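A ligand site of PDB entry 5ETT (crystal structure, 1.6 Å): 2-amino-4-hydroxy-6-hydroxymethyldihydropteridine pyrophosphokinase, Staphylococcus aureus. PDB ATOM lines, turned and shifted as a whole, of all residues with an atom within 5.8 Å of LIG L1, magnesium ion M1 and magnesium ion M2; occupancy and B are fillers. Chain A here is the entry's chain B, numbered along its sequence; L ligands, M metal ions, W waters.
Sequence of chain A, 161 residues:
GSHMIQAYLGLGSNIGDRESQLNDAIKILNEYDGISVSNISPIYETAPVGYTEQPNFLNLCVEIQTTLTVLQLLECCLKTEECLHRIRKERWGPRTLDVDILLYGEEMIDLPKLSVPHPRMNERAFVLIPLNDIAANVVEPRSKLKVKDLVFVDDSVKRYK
O of Lys 113 lies within hydrogen-bond range of O12 of LIG L1, 2.6 Å away. The guanidinium group (NH1) of Arg 88 is in salt-bridge range of an oxygen (O8) of LIG L1. The guanidinium group (NE) of Arg 120 lies within salt-bridge range of an oxygen (O3) of LIG L1, 2.8 Å away. An oxygen (O2) of LIG L1 is in hydrogen-bond range of a ring nitrogen (NE2) of His 118, at 2.8 Å. N of Ile 101 is in hydrogen-bond range of N4 of LIG L1, 3.0 Å away. A nitrogen (N3) of LIG L1 lies within hydrogen-bond range of the backbone carbonyl oxygen (O) of Ile 101, at 2.8 Å. O3 of LIG L1 lies within salt-bridge range of NH2 of Arg 124 (2.9 Å). A nitrogen (N2) of LIG L1 sits at hydrogen-bond distance from the backbone NH (N) of Ser 115 (3.0 Å). O of Ser 115 is in hydrogen-bond range of N3 of LIG L1, at 3.0 Å. An oxygen (O5) of LIG L1 lies within salt-bridge range of the guanidinium group (NH1) of Arg 95, at 3.0 Å. The guanidinium group (NH2) of Arg 86 lies within salt-bridge range of an oxygen (O8) of LIG L1, at 3.2 Å. The guanidinium group of Arg 124 sits close to a sulfur (S1) of LG2 L2, at 3.4 Å.
The side-chain carboxylate (OD1) of Asp 98 sits close to the guanidinium group (NH1) of Arg 86, at 3.0 Å. NH2 of Arg 88 is in salt-bridge range of OE1 of Glu 81, 3.9 Å away. ND1 of His 118 sits at hydrogen-bond distance from N of Arg 120. O of Leu 102 is in hydrogen-bond range of N of His 118 (3.0 Å). The guanidinium group (NH1) of Arg 86 lies within salt-bridge range of the side-chain carboxylate (OE2) of Glu 81, 3.2 Å away.
Merely in contact with LIG L1: Leu 74, Leu 78, Leu 114 and Val 116. Hydrophobic or aromatic side chains within 4 Å of LIG L1: Leu 74, Leu 78, Ile 101, Leu 114, Val 116 and His 118. Within 4 Å of LIG L1: Leu 74, Leu 78, Arg 86, Arg 88, Arg 95, Asp 98, Asp 100, Ile 101, Lys 113, Leu 114, Ser 115, Val 116, His 118, Arg 120 and Arg 124. The nearest printed residue that does not touch LIG L1 is Val 99 (4.01 Å).
Within 4 Å of magnesium ion M1: Asp 98 and Asp 100.
The nearest printed residue that does not touch magnesium ion M2 is Arg 124 (4.3 Å).
Magnesium ion M1 is bound by the side-chain carboxylate of Asp 98, an oxygen (O7) of LIG L1, water W5, the side-chain carboxylate of Asp 100, an oxygen (O4) of LIG L1 and water W8.
Magnesium ion M2 is bound by an oxygen (O1) of LIG L1 (2.0 Å), the side-chain carboxylate of Asp 98 (2.1 Å), the side-chain carboxylate of Asp 100 (2.1 Å), water W9 (2.1 Å), water W2 (2.1 Å) and an oxygen (O4) of LIG L1 (2.1 Å).
Water W5 lies within hydrogen-bond range of OE2 of Glu 81 and O of Val 99. Water W2 lies within hydrogen-bond range of N5 of LG2 L2, O5 of LIG L1 and NH1 of Arg 95. Water W6 lies within hydrogen-bond range of an oxygen (O11) of LIG L1 and the guanidinium group of Arg 88. Water W10 lies within hydrogen-bond range of OE1 of Glu 81, NH2 of Arg 88 and O9 of LIG L1.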
ATOM      1  N   LEU A  74      33.576  16.863  -4.968  1.00  0.00           N
ATOM      2  CA  LEU A  74      32.384  16.147  -4.516  1.00  0.00           C
ATOM      3  C   LEU A  74      31.472  17.066  -3.715  1.00  0.00           C
ATOM      4  O   LEU A  74      30.235  17.122  -3.976  1.00  0.00           O
ATOM      5  CB  LEU A  74      32.771  14.939  -3.693  1.00  0.00           C
ATOM      6  CG  LEU A  74      31.536  14.192  -3.194  1.00  0.00           C
ATOM      7  CD1 LEU A  74      30.764  13.529  -4.273  1.00  0.00           C
ATOM      8  CD2 LEU A  74      32.064  13.157  -2.159  1.00  0.00           C
ATOM      9  N   LEU A  78      27.503  17.800  -4.731  1.00  0.00           N
ATOM     10  CA  LEU A  78      26.361  17.540  -3.837  1.00  0.00           C
ATOM     11  C   LEU A  78      25.644  18.830  -3.463  1.00  0.00           C
ATOM     12  O   LEU A  78      24.413  18.874  -3.393  1.00  0.00           O
ATOM     13  CB  LEU A  78      26.862  16.808  -2.582  1.00  0.00           C
ATOM     14  CG  LEU A  78      27.524  15.469  -2.822  1.00  0.00           C
ATOM     15  CD1 LEU A  78      27.976  14.836  -1.487  1.00  0.00           C
ATOM     16  CD2 LEU A  78      26.716  14.495  -3.685  1.00  0.00           C
ATOM     17  N   GLU A  81      23.170  19.557  -6.256  1.00  0.00           N
ATOM     18  CA  GLU A  81      21.969  18.791  -6.083  1.00  0.00           C
ATOM     19  C   GLU A  81      20.996  19.441  -5.042  1.00  0.00           C
ATOM     20  O   GLU A  81      19.758  19.439  -5.273  1.00  0.00           O
ATOM     21  CB  GLU A  81      22.288  17.362  -5.628  1.00  0.00           C
ATOM     22  CG  GLU A  81      22.990  16.542  -6.690  1.00  0.00           C
ATOM     23  CD  GLU A  81      23.428  15.205  -6.144  1.00  0.00           C
ATOM     24  OE1 GLU A  81      23.393  14.985  -4.905  1.00  0.00           O
ATOM     25  OE2 GLU A  81      23.862  14.357  -6.995  1.00  0.00           O
ATOM     26  N   ARG A  86      16.972  18.220  -4.633  1.00  0.00           N
ATOM     27  CA  ARG A  86      16.873  16.745  -4.686  1.00  0.00           C
ATOM     28  C   ARG A  86      16.363  16.173  -3.358  1.00  0.00           C
ATOM     29  O   ARG A  86      16.869  16.537  -2.279  1.00  0.00           O
ATOM     30  CB  ARG A  86      18.194  16.208  -4.989  1.00  0.00           C
ATOM     31  CG  ARG A  86      18.066  14.640  -4.981  1.00  0.00           C
ATOM     32  CD  ARG A  86      19.157  14.052  -5.690  1.00  0.00           C
ATOM     33  NE  ARG A  86      19.285  12.628  -5.466  1.00  0.00           N
ATOM     34  CZ  ARG A  86      20.355  11.974  -5.947  1.00  0.00           C
ATOM     35  NH1 ARG A  86      21.232  12.590  -6.715  1.00  0.00           N
ATOM     36  NH2 ARG A  86      20.508  10.707  -5.674  1.00  0.00           N
ATOM     37  N   ARG A  88      15.768  12.948  -0.767  1.00  0.00           N
ATOM     38  CA  ARG A  88      16.443  11.708  -0.391  1.00  0.00           C
ATOM     39  C   ARG A  88      15.547  10.966   0.597  1.00  0.00           C
ATOM     40  O   ARG A  88      15.609  11.218   1.773  1.00  0.00           O
ATOM     41  CB  ARG A  88      17.789  12.023   0.233  1.00  0.00           C
ATOM     42  CG  ARG A  88      18.419  13.313  -0.267  1.00  0.00           C
ATOM     43  CD  ARG A  88      19.929  13.283  -0.190  1.00  0.00           C
ATOM     44  NE  ARG A  88      20.387  11.966  -0.600  1.00  0.00           N
ATOM     45  CZ  ARG A  88      21.006  11.705  -1.742  1.00  0.00           C
ATOM     46  NH1 ARG A  88      21.368  10.467  -1.973  1.00  0.00           N
ATOM     47  NH2 ARG A  88      21.340  12.682  -2.586  1.00  0.00           N
ATOM     48  N   ARG A  95      14.679  11.775  -9.293  1.00  0.00           N
ATOM     49  CA  ARG A  95      15.517  12.827  -8.722  1.00  0.00           C
ATOM     50  C   ARG A  95      15.589  13.991  -9.678  1.00  0.00           C
ATOM     51  O   ARG A  95      15.728  13.852 -10.927  1.00  0.00           O
ATOM     52  CB  ARG A  95      16.910  12.310  -8.334  1.00  0.00           C
ATOM     53  CG  ARG A  95      17.785  11.763  -9.468  1.00  0.00           C
ATOM     54  CD  ARG A  95      17.470  10.295  -9.806  1.00  0.00           C
ATOM     55  NE  ARG A  95      17.453   9.437  -8.688  1.00  0.00           N
ATOM     56  CZ  ARG A  95      18.529   8.869  -8.168  1.00  0.00           C
ATOM     57  NH1 ARG A  95      19.723   9.010  -8.767  1.00  0.00           N
ATOM     58  NH2 ARG A  95      18.412   8.213  -7.044  1.00  0.00           N
ATOM     59  N   ASP A  98      21.125  14.543 -10.345  1.00  0.00           N
ATOM     60  CA  ASP A  98      22.224  13.715  -9.868  1.00  0.00           C
ATOM     61  C   ASP A  98      23.495  14.188 -10.557  1.00  0.00           C
ATOM     62  O   ASP A  98      23.522  14.311 -11.799  1.00  0.00           O
ATOM     63  CB  ASP A  98      21.934  12.257 -10.223  1.00  0.00           C
ATOM     64  CG  ASP A  98      22.978  11.276  -9.688  1.00  0.00           C
ATOM     65  OD1 ASP A  98      23.390  11.453  -8.527  1.00  0.00           O
ATOM     66  OD2 ASP A  98      23.334  10.300 -10.474  1.00  0.00           O
ATOM     67  N   VAL A  99      24.531  14.478  -9.750  1.00  0.00           N
ATOM     68  CA  VAL A  99      25.834  14.908 -10.255  1.00  0.00           C
ATOM     69  C   VAL A  99      26.859  13.905  -9.741  1.00  0.00           C
ATOM     70  O   VAL A  99      27.158  13.871  -8.533  1.00  0.00           O
ATOM     71  CB  VAL A  99      26.225  16.356  -9.796  1.00  0.00           C
ATOM     72  CG1 VAL A  99      27.525  16.769 -10.512  1.00  0.00           C
ATOM     73  CG2 VAL A  99      25.165  17.383 -10.134  1.00  0.00           C
ATOM     74  N   ASP A 100      27.412  13.137 -10.683  1.00  0.00           N
ATOM     75  CA  ASP A 100      28.335  12.086 -10.308  1.00  0.00           C
ATOM     76  C   ASP A 100      29.703  12.368 -10.886  1.00  0.00           C
ATOM     77  O   ASP A 100      29.816  12.830 -11.995  1.00  0.00           O
ATOM     78  CB  ASP A 100      27.849  10.789 -10.891  1.00  0.00           C
ATOM     79  CG  ASP A 100      26.587  10.222 -10.192  1.00  0.00           C
ATOM     80  OD1 ASP A 100      26.261  10.736  -9.111  1.00  0.00           O
ATOM     81  OD2 ASP A 100      26.053   9.247 -10.766  1.00  0.00           O
ATOM     82  N   ILE A 101      30.751  12.166 -10.087  1.00  0.00           N
ATOM     83  CA  ILE A 101      32.098  12.306 -10.605  1.00  0.00           C
ATOM     84  C   ILE A 101      32.484  11.030 -11.316  1.00  0.00           C
ATOM     85  O   ILE A 101      32.541   9.984 -10.710  1.00  0.00           O
ATOM     86  CB  ILE A 101      33.133  12.604  -9.478  1.00  0.00           C
ATOM     87  CG1 ILE A 101      32.765  13.919  -8.715  1.00  0.00           C
ATOM     88  CG2 ILE A 101      34.522  12.701 -10.110  1.00  0.00           C
ATOM     89  CD1 ILE A 101      33.524  14.106  -7.464  1.00  0.00           C
ATOM     90  N   LEU A 102      32.767  11.151 -12.612  1.00  0.00           N
ATOM     91  CA  LEU A 102      33.066   9.954 -13.442  1.00  0.00           C
ATOM     92  C   LEU A 102      34.580   9.714 -13.427  1.00  0.00           C
ATOM     93  O   LEU A 102      35.005   8.587 -13.144  1.00  0.00           O
ATOM     94  CB  LEU A 102      32.556  10.162 -14.859  1.00  0.00           C
ATOM     95  CG  LEU A 102      31.048  10.417 -14.953  1.00  0.00           C
ATOM     96  CD1 LEU A 102      30.650  10.705 -16.402  1.00  0.00           C
ATOM     97  CD2 LEU A 102      30.243   9.244 -14.378  1.00  0.00           C
ATOM     98  N   PRO A 112      35.379   5.649   1.573  1.00  0.00           N
ATOM     99  CA  PRO A 112      34.005   5.379   1.885  1.00  0.00           C
ATOM    100  C   PRO A 112      33.004   6.279   1.210  1.00  0.00           C
ATOM    101  O   PRO A 112      32.010   5.759   0.715  1.00  0.00           O
ATOM    102  CB  PRO A 112      33.941   5.495   3.393  1.00  0.00           C
ATOM    103  CG  PRO A 112      35.280   5.065   3.801  1.00  0.00           C
ATOM    104  CD  PRO A 112      36.200   5.707   2.819  1.00  0.00           C
ATOM    105  N   LYS A 113      33.258   7.557   1.132  1.00  0.00           N
ATOM    106  CA  LYS A 113      32.341   8.489   0.539  1.00  0.00           C
ATOM    107  C   LYS A 113      32.579   8.757  -0.949  1.00  0.00           C
ATOM    108  O   LYS A 113      31.847   9.568  -1.510  1.00  0.00           O
ATOM    109  CB  LYS A 113      32.271   9.763   1.366  1.00  0.00           C
ATOM    110  CG  LYS A 113      33.395  10.809   1.218  1.00  0.00           C
ATOM    111  CD  LYS A 113      33.542  11.872   2.357  1.00  0.00           C
ATOM    112  CE  LYS A 113      32.380  12.855   2.350  1.00  0.00           C
ATOM    113  NZ  LYS A 113      32.471  13.879   3.436  1.00  0.00           N
ATOM    114  N   LEU A 114      33.603   8.187  -1.570  1.00  0.00           N
ATOM    115  CA  LEU A 114      33.986   8.588  -2.910  1.00  0.00           C
ATOM    116  C   LEU A 114      34.719   7.474  -3.614  1.00  0.00           C
ATOM    117  O   LEU A 114      35.846   7.135  -3.179  1.00  0.00           O
ATOM    118  CB  LEU A 114      34.816   9.859  -2.898  1.00  0.00           C
ATOM    119  CG  LEU A 114      35.254  10.443  -4.234  1.00  0.00           C
ATOM    120  CD1 LEU A 114      34.074  10.760  -5.133  1.00  0.00           C
ATOM    121  CD2 LEU A 114      36.163  11.628  -4.073  1.00  0.00           C
ATOM    122  N   SER A 115      34.219   7.051  -4.774  1.00  0.00           N
ATOM    123  CA  SER A 115      34.924   6.102  -5.627  1.00  0.00           C
ATOM    124  C   SER A 115      35.053   6.669  -7.017  1.00  0.00           C
ATOM    125  O   SER A 115      34.010   6.996  -7.614  1.00  0.00           O
ATOM    126  CB  SER A 115      34.181   4.797  -5.731  1.00  0.00           C
ATOM    127  OG  SER A 115      33.941   4.269  -4.454  1.00  0.00           O
ATOM    128  N   VAL A 116      36.266   6.854  -7.534  1.00  0.00           N
ATOM    129  CA  VAL A 116      36.557   7.430  -8.822  1.00  0.00           C
ATOM    130  C   VAL A 116      37.654   6.634  -9.476  1.00  0.00           C
ATOM    131  O   VAL A 116      38.673   6.365  -8.760  1.00  0.00           O
ATOM    132  CB  VAL A 116      36.986   8.927  -8.711  1.00  0.00           C
ATOM    133  CG1 VAL A 116      37.382   9.433 -10.092  1.00  0.00           C
ATOM    134  CG2 VAL A 116      35.888   9.768  -8.016  1.00  0.00           C
ATOM    135  N   PRO A 117      37.535   6.198 -10.720  1.00  0.00           N
ATOM    136  CA  PRO A 117      36.387   6.330 -11.589  1.00  0.00           C
ATOM    137  C   PRO A 117      35.140   5.793 -10.983  1.00  0.00           C
ATOM    138  O   PRO A 117      35.158   4.856 -10.148  1.00  0.00           O
ATOM    139  CB  PRO A 117      36.775   5.538 -12.793  1.00  0.00           C
ATOM    140  CG  PRO A 117      38.258   5.758 -12.871  1.00  0.00           C
ATOM    141  CD  PRO A 117      38.685   5.614 -11.475  1.00  0.00           C
ATOM    142  N   HIS A 118      33.998   6.364 -11.382  1.00  0.00           N
ATOM    143  CA  HIS A 118      32.711   5.884 -10.871  1.00  0.00           C
ATOM    144  C   HIS A 118      32.625   4.382 -11.052  1.00  0.00           C
ATOM    145  O   HIS A 118      32.902   3.876 -12.138  1.00  0.00           O
ATOM    146  CB  HIS A 118      31.590   6.644 -11.541  1.00  0.00           C
ATOM    147  CG  HIS A 118      30.266   6.365 -10.906  1.00  0.00           C
ATOM    148  ND1 HIS A 118      29.648   5.152 -11.028  1.00  0.00           N
ATOM    149  CD2 HIS A 118      29.488   7.071 -10.052  1.00  0.00           C
ATOM    150  CE1 HIS A 118      28.525   5.129 -10.313  1.00  0.00           C
ATOM    151  NE2 HIS A 118      28.434   6.305  -9.690  1.00  0.00           N
ATOM    152  N   PRO A 119      32.196   3.637  -9.997  1.00  0.00           N
ATOM    153  CA  PRO A 119      32.335   2.175 -10.033  1.00  0.00           C
ATOM    154  C   PRO A 119      31.487   1.529 -11.032  1.00  0.00           C
ATOM    155  O   PRO A 119      31.662   0.347 -11.347  1.00  0.00           O
ATOM    156  CB  PRO A 119      31.874   1.726  -8.664  1.00  0.00           C
ATOM    157  CG  PRO A 119      31.442   2.885  -7.900  1.00  0.00           C
ATOM    158  CD  PRO A 119      31.849   4.123  -8.662  1.00  0.00           C
ATOM    159  N   ARG A 120      30.450   2.199 -11.525  1.00  0.00           N
ATOM    160  CA  ARG A 120      29.529   1.603 -12.505  1.00  0.00           C
ATOM    161  C   ARG A 120      29.626   2.165 -13.919  1.00  0.00           C
ATOM    162  O   ARG A 120      28.888   1.678 -14.796  1.00  0.00           O
ATOM    163  CB  ARG A 120      28.079   1.719 -11.989  1.00  0.00           C
ATOM    164  CG  ARG A 120      27.829   0.772 -10.810  1.00  0.00           C
ATOM    165  CD  ARG A 120      26.546   1.028 -10.026  1.00  0.00           C
ATOM    166  NE  ARG A 120      26.636   2.180  -9.134  1.00  0.00           N
ATOM    167  CZ  ARG A 120      27.285   2.194  -7.984  1.00  0.00           C
ATOM    168  NH1 ARG A 120      27.927   1.100  -7.527  1.00  0.00           N
ATOM    169  NH2 ARG A 120      27.356   3.277  -7.220  1.00  0.00           N
ATOM    170  N   ARG A 124      27.649   1.362 -18.290  1.00  0.00           N
ATOM    171  CA  ARG A 124      26.462   2.217 -18.387  1.00  0.00           C
ATOM    172  C   ARG A 124      26.455   3.008 -19.711  1.00  0.00           C
ATOM    173  O   ARG A 124      27.206   3.883 -19.861  1.00  0.00           O
ATOM    174  CB  ARG A 124      26.446   3.223 -17.254  1.00  0.00           C
ATOM    175  CG  ARG A 124      25.856   2.659 -15.989  1.00  0.00           C
ATOM    176  CD  ARG A 124      26.072   3.538 -14.769  1.00  0.00           C
ATOM    177  NE  ARG A 124      25.256   3.073 -13.662  1.00  0.00           N
ATOM    178  CZ  ARG A 124      25.042   3.765 -12.566  1.00  0.00           C
ATOM    179  NH1 ARG A 124      25.632   4.949 -12.384  1.00  0.00           N
ATOM    180  NH2 ARG A 124      24.261   3.246 -11.645  1.00  0.00           N
ATOM    181  N   PHE A 126      24.236   5.120 -20.588  1.00  0.00           N
ATOM    182  CA  PHE A 126      23.801   6.502 -20.341  1.00  0.00           C
ATOM    183  C   PHE A 126      24.968   7.385 -19.886  1.00  0.00           C
ATOM    184  O   PHE A 126      24.833   8.637 -19.911  1.00  0.00           O
ATOM    185  CB  PHE A 126      22.664   6.585 -19.343  1.00  0.00           C
ATOM    186  CG  PHE A 126      23.027   6.331 -17.905  1.00  0.00           C
ATOM    187  CD1 PHE A 126      23.540   7.334 -17.158  1.00  0.00           C
ATOM    188  CD2 PHE A 126      22.799   5.097 -17.298  1.00  0.00           C
ATOM    189  CE1 PHE A 126      23.780   7.137 -15.771  1.00  0.00           C
ATOM    190  CE2 PHE A 126      23.064   4.873 -15.955  1.00  0.00           C
ATOM    191  CZ  PHE A 126      23.569   5.882 -15.198  1.00  0.00           C
HETATM  192  P1  LIG L   1      25.084   5.757  -8.746  1.00  0.00           P
HETATM  193  O1  LIG L   1      24.989   6.582 -10.044  1.00  0.00           O
HETATM  194  O2  LIG L   1      26.308   5.960  -7.918  1.00  0.00           O
HETATM  195  O3  LIG L   1      24.822   4.274  -8.965  1.00  0.00           O
HETATM  196  P2  LIG L   1      23.466   7.652  -7.248  1.00  0.00           P
HETATM  197  O4  LIG L   1      24.236   8.611  -8.115  1.00  0.00           O
HETATM  198  O5  LIG L   1      21.972   7.782  -7.264  1.00  0.00           O
HETATM  199  O6  LIG L   1      23.836   6.196  -7.795  1.00  0.00           O
HETATM  200  P3  LIG L   1      23.758   9.242  -4.801  1.00  0.00           P
HETATM  201  O7  LIG L   1      23.815  10.343  -5.790  1.00  0.00           O
HETATM  202  O8  LIG L   1      22.587   9.128  -3.885  1.00  0.00           O
HETATM  203  C1  LIG L   1      24.168   7.674  -5.615  1.00  0.00           C
HETATM  204  O9  LIG L   1      25.006   9.546  -3.842  1.00  0.00           O
HETATM  205  C2  LIG L   1      25.316   8.837  -2.672  1.00  0.00           C
HETATM  206  C3  LIG L   1      26.796   9.079  -2.261  1.00  0.00           C
HETATM  207  O10 LIG L   1      27.623   8.492  -3.240  1.00  0.00           O
HETATM  208  C4  LIG L   1      27.261  10.503  -2.216  1.00  0.00           C
HETATM  209  O11 LIG L   1      26.878  11.138  -1.016  1.00  0.00           O
HETATM  210  C5  LIG L   1      28.763  10.337  -2.285  1.00  0.00           C
HETATM  211  O12 LIG L   1      29.431  10.362  -0.978  1.00  0.00           O
HETATM  212  C6  LIG L   1      28.907   8.953  -2.834  1.00  0.00           C
HETATM  213  N1  LIG L   1      29.786   8.774  -4.020  1.00  0.00           N
HETATM  214  C7  LIG L   1      30.731   7.765  -4.172  1.00  0.00           C
HETATM  215  N2  LIG L   1      31.386   7.900  -5.346  1.00  0.00           N
HETATM  216  C8  LIG L   1      30.802   9.012  -5.935  1.00  0.00           C
HETATM  217  C9  LIG L   1      31.076   9.609  -7.188  1.00  0.00           C
HETATM  218  N3  LIG L   1      32.025   9.135  -8.067  1.00  0.00           N
HETATM  219  N4  LIG L   1      30.348  10.700  -7.529  1.00  0.00           N
HETATM  220  C10 LIG L   1      29.418  11.129  -6.666  1.00  0.00           C
HETATM  221  N5  LIG L   1      29.077  10.665  -5.436  1.00  0.00           N
HETATM  222  C11 LIG L   1      29.819   9.576  -5.148  1.00  0.00           C
HETATM  223  C1  LG2 L   2      14.773   6.389 -10.335  1.00  0.00           C
HETATM  224  C2  LG2 L   2      16.307   4.787 -11.213  1.00  0.00           C
HETATM  225  C3  LG2 L   2      17.464   4.051 -11.118  1.00  0.00           C
HETATM  226  C4  LG2 L   2      16.675   5.645  -9.046  1.00  0.00           C
HETATM  227  C5  LG2 L   2      15.921   5.610 -10.186  1.00  0.00           C
HETATM  228  C6  LG2 L   2      18.290   4.045  -9.981  1.00  0.00           C
HETATM  229  C7  LG2 L   2      20.698   6.571 -13.699  1.00  0.00           C
HETATM  230  C8  LG2 L   2      17.803   4.851  -8.967  1.00  0.00           C
HETATM  231  C9  LG2 L   2      20.195   5.344 -14.040  1.00  0.00           C
HETATM  232  C10 LG2 L   2      20.749   7.649 -14.624  1.00  0.00           C
HETATM  233  C11 LG2 L   2      19.690   5.978 -16.095  1.00  0.00           C
HETATM  234  C12 LG2 L   2      20.919   5.323 -11.989  1.00  0.00           C
HETATM  235  C13 LG2 L   2      19.682   3.359  -9.909  1.00  0.00           C
HETATM  236  N1  LG2 L   2      13.858   7.097 -10.412  1.00  0.00           N
HETATM  237  N2  LG2 L   2      19.655   5.018 -15.216  1.00  0.00           N
HETATM  238  N3  LG2 L   2      20.341   4.519 -12.961  1.00  0.00           N
HETATM  239  N4  LG2 L   2      20.202   7.262 -15.829  1.00  0.00           N
HETATM  240  N5  LG2 L   2      21.182   6.534 -12.402  1.00  0.00           N
HETATM  241  N6  LG2 L   2      19.254   5.876 -17.359  1.00  0.00           N
HETATM  242  O1  LG2 L   2      21.209   8.817 -14.449  1.00  0.00           O
HETATM  243  F1  LG2 L   2      18.461   4.990  -7.790  1.00  0.00           F
HETATM  244  S1  LG2 L   2      21.302   4.551 -10.449  1.00  0.00           S
HETATM  245 MG    MG M   1      24.904  10.528  -7.521  1.00  0.00          MG
HETATM  246 MG    MG M   2      24.188   8.442 -10.253  1.00  0.00          MG
HETATM  247  O   HOH W   1      30.470   5.929  -1.488  1.00  0.00           O
HETATM  248  O   HOH W   2      22.233   7.633 -10.057  1.00  0.00           O
HETATM  249  O   HOH W   3      27.720   7.172  -6.247  1.00  0.00           O
HETATM  250  O   HOH W   4      28.869  12.349   1.092  1.00  0.00           O
HETATM  251  O   HOH W   5      25.635  12.346  -6.857  1.00  0.00           O
HETATM  252  O   HOH W   6      24.453  12.134  -1.443  1.00  0.00           O
HETATM  253  O   HOH W   7      27.129   5.602  -4.022  1.00  0.00           O
HETATM  254  O   HOH W   8      26.545   9.621  -6.522  1.00  0.00           O
HETATM  255  O   HOH W   9      23.862   8.096 -12.317  1.00  0.00           O
HETATM  256  O   HOH W  10      23.598  12.537  -4.041  1.00  0.00           O
HETATM  257  O   HOH W  11      23.186   2.555  -7.768  1.00  0.00           O
HETATM  258  O   HOH W  12      29.898   5.721  -6.537  1.00  0.00           O
